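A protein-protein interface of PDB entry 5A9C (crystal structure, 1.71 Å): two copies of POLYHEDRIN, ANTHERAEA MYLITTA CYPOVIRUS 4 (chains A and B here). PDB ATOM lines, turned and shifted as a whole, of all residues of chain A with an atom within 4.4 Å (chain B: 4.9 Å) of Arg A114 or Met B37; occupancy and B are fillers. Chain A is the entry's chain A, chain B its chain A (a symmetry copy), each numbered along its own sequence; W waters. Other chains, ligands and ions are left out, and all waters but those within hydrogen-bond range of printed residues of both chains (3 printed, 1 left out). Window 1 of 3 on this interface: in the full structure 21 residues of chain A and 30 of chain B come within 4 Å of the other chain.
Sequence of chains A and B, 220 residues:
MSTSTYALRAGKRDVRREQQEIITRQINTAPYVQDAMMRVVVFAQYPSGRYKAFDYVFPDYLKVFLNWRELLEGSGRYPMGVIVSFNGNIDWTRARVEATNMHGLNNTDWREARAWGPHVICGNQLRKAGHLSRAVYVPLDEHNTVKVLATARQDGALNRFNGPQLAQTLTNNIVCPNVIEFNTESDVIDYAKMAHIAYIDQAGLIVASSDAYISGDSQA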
ATOM      1  N   ASN A 106      10.476  -6.298  -1.779  1.00  0.00           N
ATOM      2  CA  ASN A 106       9.306  -5.616  -2.328  1.00  0.00           C
ATOM      3  C   ASN A 106       9.415  -4.095  -2.202  1.00  0.00           C
ATOM      4  O   ASN A 106       8.473  -3.360  -2.501  1.00  0.00           O
ATOM      5  CB  ASN A 106       7.998  -6.146  -1.722  1.00  0.00           C
ATOM      6  CG  ASN A 106       8.028  -6.199  -0.207  1.00  0.00           C
ATOM      7  OD1 ASN A 106       8.526  -5.287   0.452  1.00  0.00           O
ATOM      8  ND2 ASN A 106       7.488  -7.274   0.354  1.00  0.00           N
ATOM      9  N   TRP A 110      15.851  -1.898   1.276  1.00  0.00           N
ATOM     10  CA  TRP A 110      15.471  -2.963   2.200  1.00  0.00           C
ATOM     11  C   TRP A 110      14.972  -2.421   3.536  1.00  0.00           C
ATOM     12  O   TRP A 110      14.169  -3.065   4.213  1.00  0.00           O
ATOM     13  CB  TRP A 110      16.636  -3.940   2.430  1.00  0.00           C
ATOM     14  CG  TRP A 110      17.736  -3.401   3.309  1.00  0.00           C
ATOM     15  CD1 TRP A 110      18.875  -2.776   2.903  1.00  0.00           C
ATOM     16  CD2 TRP A 110      17.797  -3.452   4.745  1.00  0.00           C
ATOM     17  NE1 TRP A 110      19.642  -2.429   3.992  1.00  0.00           N
ATOM     18  CE2 TRP A 110      19.004  -2.831   5.133  1.00  0.00           C
ATOM     19  CE3 TRP A 110      16.949  -3.956   5.735  1.00  0.00           C
ATOM     20  CZ2 TRP A 110      19.381  -2.701   6.469  1.00  0.00           C
ATOM     21  CZ3 TRP A 110      17.328  -3.826   7.064  1.00  0.00           C
ATOM     22  CH2 TRP A 110      18.534  -3.206   7.418  1.00  0.00           C
ATOM     23  N   ARG A 111      15.443  -1.234   3.906  1.00  0.00           N
ATOM     24  CA  ARG A 111      15.066  -0.616   5.174  1.00  0.00           C
ATOM     25  C   ARG A 111      13.584  -0.250   5.227  1.00  0.00           C
ATOM     26  O   ARG A 111      13.034  -0.014   6.301  1.00  0.00           O
ATOM     27  CB  ARG A 111      15.929   0.619   5.442  1.00  0.00           C
ATOM     28  CG  ARG A 111      17.401   0.300   5.661  1.00  0.00           C
ATOM     29  CD  ARG A 111      18.257   1.559   5.663  1.00  0.00           C
ATOM     30  NE  ARG A 111      18.157   2.277   4.396  1.00  0.00           N
ATOM     31  CZ  ARG A 111      18.905   3.326   4.064  1.00  0.00           C
ATOM     32  NH1 ARG A 111      19.826   3.785   4.905  1.00  0.00           N
ATOM     33  NH2 ARG A 111      18.734   3.913   2.888  1.00  0.00           N
ATOM     34  N   GLU A 112      12.940  -0.206   4.066  1.00  0.00           N
ATOM     35  CA  GLU A 112      11.508   0.072   4.015  1.00  0.00           C
ATOM     36  C   GLU A 112      10.735  -1.042   3.307  1.00  0.00           C
ATOM     37  O   GLU A 112       9.576  -0.874   2.935  1.00  0.00           O
ATOM     38  CB  GLU A 112      11.246   1.447   3.396  1.00  0.00           C
ATOM     39  CG  GLU A 112      11.843   2.577   4.230  1.00  0.00           C
ATOM     40  CD  GLU A 112      11.487   3.957   3.722  1.00  0.00           C
ATOM     41  OE1 GLU A 112      11.462   4.152   2.493  1.00  0.00           O
ATOM     42  OE2 GLU A 112      11.244   4.852   4.558  1.00  0.00           O
ATOM     43  N   ALA A 113      11.389  -2.188   3.144  1.00  0.00           N
ATOM     44  CA  ALA A 113      10.740  -3.377   2.611  1.00  0.00           C
ATOM     45  C   ALA A 113      10.108  -4.152   3.762  1.00  0.00           C
ATOM     46  O   ALA A 113      10.473  -3.952   4.919  1.00  0.00           O
ATOM     47  CB  ALA A 113      11.742  -4.240   1.882  1.00  0.00           C
ATOM     48  N   ARG A 114       9.168  -5.037   3.440  1.00  0.00           N
ATOM     49  CA  ARG A 114       8.473  -5.825   4.455  1.00  0.00           C
ATOM     50  C   ARG A 114       8.287  -7.271   3.998  1.00  0.00           C
ATOM     51  O   ARG A 114       8.571  -7.608   2.851  1.00  0.00           O
ATOM     52  CB  ARG A 114       7.109  -5.209   4.782  1.00  0.00           C
ATOM     53  CG  ARG A 114       7.125  -4.166   5.900  1.00  0.00           C
ATOM     54  CD  ARG A 114       7.467  -2.773   5.392  1.00  0.00           C
ATOM     55  NE  ARG A 114       7.389  -1.787   6.467  1.00  0.00           N
ATOM     56  CZ  ARG A 114       8.427  -1.402   7.204  1.00  0.00           C
ATOM     57  NH1 ARG A 114       9.632  -1.908   6.975  1.00  0.00           N
ATOM     58  NH2 ARG A 114       8.261  -0.504   8.165  1.00  0.00           N
ATOM     59  N   ALA A 115       7.800  -8.120   4.897  1.00  0.00           N
ATOM     60  CA  ALA A 115       7.587  -9.528   4.577  1.00  0.00           C
ATOM     61  C   ALA A 115       6.706  -9.672   3.339  1.00  0.00           C
ATOM     62  O   ALA A 115       6.945 -10.534   2.496  1.00  0.00           O
ATOM     63  CB  ALA A 115       6.971 -10.258   5.765  1.00  0.00           C
ATOM     64  N   TRP A 116       5.688  -8.822   3.241  1.00  0.00           N
ATOM     65  CA  TRP A 116       4.835  -8.766   2.057  1.00  0.00           C
ATOM     66  C   TRP A 116       4.521  -7.314   1.693  1.00  0.00           C
ATOM     67  O   TRP A 116       4.453  -6.450   2.567  1.00  0.00           O
ATOM     68  CB  TRP A 116       3.552  -9.571   2.271  1.00  0.00           C
ATOM     69  CG  TRP A 116       3.822 -11.020   2.540  1.00  0.00           C
ATOM     70  CD1 TRP A 116       3.905 -11.625   3.759  1.00  0.00           C
ATOM     71  CD2 TRP A 116       4.077 -12.041   1.567  1.00  0.00           C
ATOM     72  NE1 TRP A 116       4.188 -12.961   3.607  1.00  0.00           N
ATOM     73  CE2 TRP A 116       4.295 -13.243   2.270  1.00  0.00           C
ATOM     74  CE3 TRP A 116       4.133 -12.058   0.170  1.00  0.00           C
ATOM     75  CZ2 TRP A 116       4.565 -14.447   1.625  1.00  0.00           C
ATOM     76  CZ3 TRP A 116       4.405 -13.255  -0.469  1.00  0.00           C
ATOM     77  CH2 TRP A 116       4.615 -14.432   0.257  1.00  0.00           C
ATOM     78  N   ALA B  30      11.895   2.530  10.053  1.00  0.00           N
ATOM     79  CA  ALA B  30      11.089   1.513   9.380  1.00  0.00           C
ATOM     80  C   ALA B  30      11.533   0.074   9.684  1.00  0.00           C
ATOM     81  O   ALA B  30      10.698  -0.818   9.816  1.00  0.00           O
ATOM     82  CB  ALA B  30      11.053   1.762   7.872  1.00  0.00           C
ATOM     83  N   PRO B  31      12.851  -0.161   9.790  1.00  0.00           N
ATOM     84  CA  PRO B  31      13.301  -1.529  10.075  1.00  0.00           C
ATOM     85  C   PRO B  31      12.859  -2.064  11.442  1.00  0.00           C
ATOM     86  O   PRO B  31      13.004  -3.261  11.689  1.00  0.00           O
ATOM     87  CB  PRO B  31      14.828  -1.408  10.025  1.00  0.00           C
ATOM     88  CG  PRO B  31      15.077  -0.248   9.118  1.00  0.00           C
ATOM     89  CD  PRO B  31      13.975   0.719   9.428  1.00  0.00           C
ATOM     90  N   VAL B  33       9.730  -1.855  12.642  1.00  0.00           N
ATOM     91  CA  VAL B  33       8.354  -2.335  12.566  1.00  0.00           C
ATOM     92  C   VAL B  33       8.346  -3.865  12.550  1.00  0.00           C
ATOM     93  O   VAL B  33       9.264  -4.490  12.021  1.00  0.00           O
ATOM     94  CB  VAL B  33       7.624  -1.763  11.331  1.00  0.00           C
ATOM     95  CG1 VAL B  33       6.223  -2.345  11.209  1.00  0.00           C
ATOM     96  CG2 VAL B  33       7.559  -0.245  11.420  1.00  0.00           C
ATOM     97  N   ASP B  35       6.994  -6.387  11.015  1.00  0.00           N
ATOM     98  CA  ASP B  35       7.144  -7.200   9.813  1.00  0.00           C
ATOM     99  C   ASP B  35       8.209  -6.634   8.883  1.00  0.00           C
ATOM    100  O   ASP B  35       8.216  -6.915   7.682  1.00  0.00           O
ATOM    101  CB  ASP B  35       5.811  -7.343   9.074  1.00  0.00           C
ATOM    102  CG  ASP B  35       5.382  -6.063   8.389  1.00  0.00           C
ATOM    103  OD1 ASP B  35       5.650  -4.972   8.938  1.00  0.00           O
ATOM    104  OD2 ASP B  35       4.778  -6.150   7.297  1.00  0.00           O
ATOM    105  N   ALA B  36       9.110  -5.837   9.445  1.00  0.00           N
ATOM    106  CA  ALA B  36      10.198  -5.261   8.670  1.00  0.00           C
ATOM    107  C   ALA B  36      11.168  -6.345   8.224  1.00  0.00           C
ATOM    108  O   ALA B  36      11.230  -7.426   8.816  1.00  0.00           O
ATOM    109  CB  ALA B  36      10.929  -4.195   9.481  1.00  0.00           C
ATOM    110  N   MET B  37      11.920  -6.052   7.171  1.00  0.00           N
ATOM    111  CA  MET B  37      12.944  -6.967   6.702  1.00  0.00           C
ATOM    112  C   MET B  37      14.255  -6.739   7.440  1.00  0.00           C
ATOM    113  O   MET B  37      14.587  -5.613   7.816  1.00  0.00           O
ATOM    114  CB  MET B  37      13.152  -6.812   5.193  1.00  0.00           C
ATOM    115  CG  MET B  37      11.935  -7.182   4.363  1.00  0.00           C
ATOM    116  SD  MET B  37      11.467  -8.915   4.536  1.00  0.00           S
ATOM    117  CE  MET B  37      12.844  -9.707   3.714  1.00  0.00           C
ATOM    118  N   MET B  38      14.986  -7.825   7.663  1.00  0.00           N
ATOM    119  CA  MET B  38      16.353  -7.749   8.150  1.00  0.00           C
ATOM    120  C   MET B  38      17.273  -8.205   7.028  1.00  0.00           C
ATOM    121  O   MET B  38      16.824  -8.818   6.058  1.00  0.00           O
ATOM    122  CB  MET B  38      16.540  -8.626   9.391  1.00  0.00           C
ATOM    123  CG  MET B  38      15.912  -8.054  10.654  1.00  0.00           C
ATOM    124  SD  MET B  38      15.839  -9.257  11.997  1.00  0.00           S
ATOM    125  CE  MET B  38      14.586 -10.365  11.360  1.00  0.00           C
ATOM    126  N   ARG B  39      18.558  -7.896   7.143  1.00  0.00           N
ATOM    127  CA  ARG B  39      19.493  -8.270   6.097  1.00  0.00           C
ATOM    128  C   ARG B  39      20.819  -8.713   6.680  1.00  0.00           C
ATOM    129  O   ARG B  39      21.494  -7.950   7.373  1.00  0.00           O
ATOM    130  CB  ARG B  39      19.704  -7.112   5.118  1.00  0.00           C
ATOM    131  CG  ARG B  39      20.398  -7.522   3.828  1.00  0.00           C
ATOM    132  CD  ARG B  39      20.299  -6.420   2.792  1.00  0.00           C
ATOM    133  NE  ARG B  39      20.732  -6.865   1.472  1.00  0.00           N
ATOM    134  CZ  ARG B  39      20.502  -6.190   0.351  1.00  0.00           C
ATOM    135  NH1 ARG B  39      19.836  -5.042   0.391  1.00  0.00           N
ATOM    136  NH2 ARG B  39      20.929  -6.664  -0.812  1.00  0.00           N
ATOM    137  N   VAL B  57      17.852 -11.761   2.939  1.00  0.00           N
ATOM    138  CA  VAL B  57      16.834 -10.879   3.497  1.00  0.00           C
ATOM    139  C   VAL B  57      15.695 -11.724   4.057  1.00  0.00           C
ATOM    140  O   VAL B  57      15.292 -12.717   3.451  1.00  0.00           O
ATOM    141  CB  VAL B  57      16.320  -9.842   2.479  1.00  0.00           C
ATOM    142  CG1 VAL B  57      17.467  -8.960   2.009  1.00  0.00           C
ATOM    143  CG2 VAL B  57      15.652 -10.520   1.293  1.00  0.00           C
ATOM    144  N   PHE B  58      15.192 -11.325   5.221  1.00  0.00           N
ATOM    145  CA  PHE B  58      14.253 -12.138   5.990  1.00  0.00           C
ATOM    146  C   PHE B  58      13.585 -11.278   7.055  1.00  0.00           C
ATOM    147  O   PHE B  58      14.212 -10.372   7.600  1.00  0.00           O
ATOM    148  CB  PHE B  58      15.005 -13.282   6.671  1.00  0.00           C
ATOM    149  CG  PHE B  58      16.067 -12.814   7.630  1.00  0.00           C
ATOM    150  CD1 PHE B  58      17.292 -12.364   7.160  1.00  0.00           C
ATOM    151  CD2 PHE B  58      15.834 -12.805   8.993  1.00  0.00           C
ATOM    152  CE1 PHE B  58      18.268 -11.924   8.035  1.00  0.00           C
ATOM    153  CE2 PHE B  58      16.807 -12.369   9.875  1.00  0.00           C
ATOM    154  CZ  PHE B  58      18.027 -11.928   9.393  1.00  0.00           C
ATOM    155  N   PRO B  59      12.313 -11.564   7.363  1.00  0.00           N
ATOM    156  CA  PRO B  59      11.538 -10.735   8.294  1.00  0.00           C
ATOM    157  C   PRO B  59      11.615 -11.117   9.777  1.00  0.00           C
ATOM    158  O   PRO B  59      11.390 -10.246  10.618  1.00  0.00           O
ATOM    159  CB  PRO B  59      10.105 -10.916   7.795  1.00  0.00           C
ATOM    160  CG  PRO B  59      10.093 -12.297   7.240  1.00  0.00           C
ATOM    161  CD  PRO B  59      11.460 -12.510   6.622  1.00  0.00           C
ATOM    162  N   GLY B  88      19.500  -4.523  10.680  1.00  0.00           N
ATOM    163  CA  GLY B  88      18.085  -4.455  10.994  1.00  0.00           C
ATOM    164  C   GLY B  88      17.796  -4.507  12.482  1.00  0.00           C
ATOM    165  O   GLY B  88      18.691  -4.334  13.314  1.00  0.00           O
HETATM  166  O   HOH W   1      18.307  -2.306  -0.355  1.00  0.00           O
HETATM  167  O   HOH W   2       4.439  -8.059   5.782  1.00  0.00           O
HETATM  168  O   HOH W   3       4.766  -2.627   8.065  1.00  0.00           O
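CZ3 of Trp A110 touches O of Met B37, at 3.4 Å.
Arg B39 touches Trp A110 (NH1 to CD1, 3.5 Å).
Trp A110 touches Gly B88.
Arg A111 touches Ala B30.
CG of Glu A112 touches CB of Ala B30, 3.8 Å away.
O of Ala A113 touches CA of Ala B36 (3.98 Å).
NH2 of Arg A114 touches CG2 of Val B33, at 3.3 Å.
Arg A114 touches Asp B35 (CG to OD2, 3.4 Å).
Ala B36 touches Arg A114.
CB of Pro B59 touches CB of Ala A115, at 3.8 Å.
Asn A106 touches none of the printed residues of chain B.
Printed residues of chain B within 4 Å of Glu A112: Ala B30.
Of the printed residues of chain B, Ala A113 touches Ala B36 and Met B37.
Arg A114 touches just these residues of chain B: Ala B30 (3.0 Å), Val B33 (3.3 Å), Asp B35 (3.4 Å), Ala B36 (3.6 Å) and Met B37 (3.6 Å).
The nearest residue of chain B that does not touch Arg A114 is Pro B31 (4.6 Å).
The nearest printed residue of chain A that does not touch Met B37 is Asn A106 (5.5 Å).
The nearest printed residue of chain A that does not touch Arg B39 is Arg A111 (6.8 Å).
The backbone NH (N) of Ala A115 sits at hydrogen-bond distance from the backbone carbonyl oxygen (O) of Asp B35 (3.1 Å).
NH2 of Arg A114 sits at hydrogen-bond distance from O of Ala B30.
The backbone carbonyl oxygen of Arg A111 lies close to the backbone nitrogen of Pro B31.
The backbone carbonyl oxygen of Ala A113 lies within hydrogen-bond range of the backbone NH of Met B37 (3.4 Å).
The backbone NH (N) of Ala A115 sits at hydrogen-bond distance from the side-chain sulfur (SD) of Met B37, 3.8 Å away.
SD of Met B37 lies close to O of Arg A114 (3.6 Å).
Water W2 lies within hydrogen-bond range of OD2 of Asp B35 (2.5 Å), N of Trp A116 (2.9 Å) and N of Ala A115 (3.5 Å).
Water W3 lies within hydrogen-bond range of OD1 of Asp B35 and NE of Arg A114.
Water W1 lies within hydrogen-bond range of N of Trp A110 (3.0 Å) and NH1 of Arg B39 (3.2 Å).
Of the 8 printed residues of chain A, 6 touch a printed residue of chain B.
Printed residues of chain A that touch a printed residue of chain B: Trp A110, Arg A111, Glu A112, Ala A113, Arg A114 and Ala A115.
Hydrophobic or aromatic side chains of chain A that line the printed part of chain B: Trp A110, Ala A113 and Ala A115.
ND2 of Asn A106 is in hydrogen-bond range of O of Arg A114 (2.7 Å).
No position is printed for both chains.
Of the 16 pairs that touch across the chains among the printed residues, none has its exchanged pair printed and touching as well.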
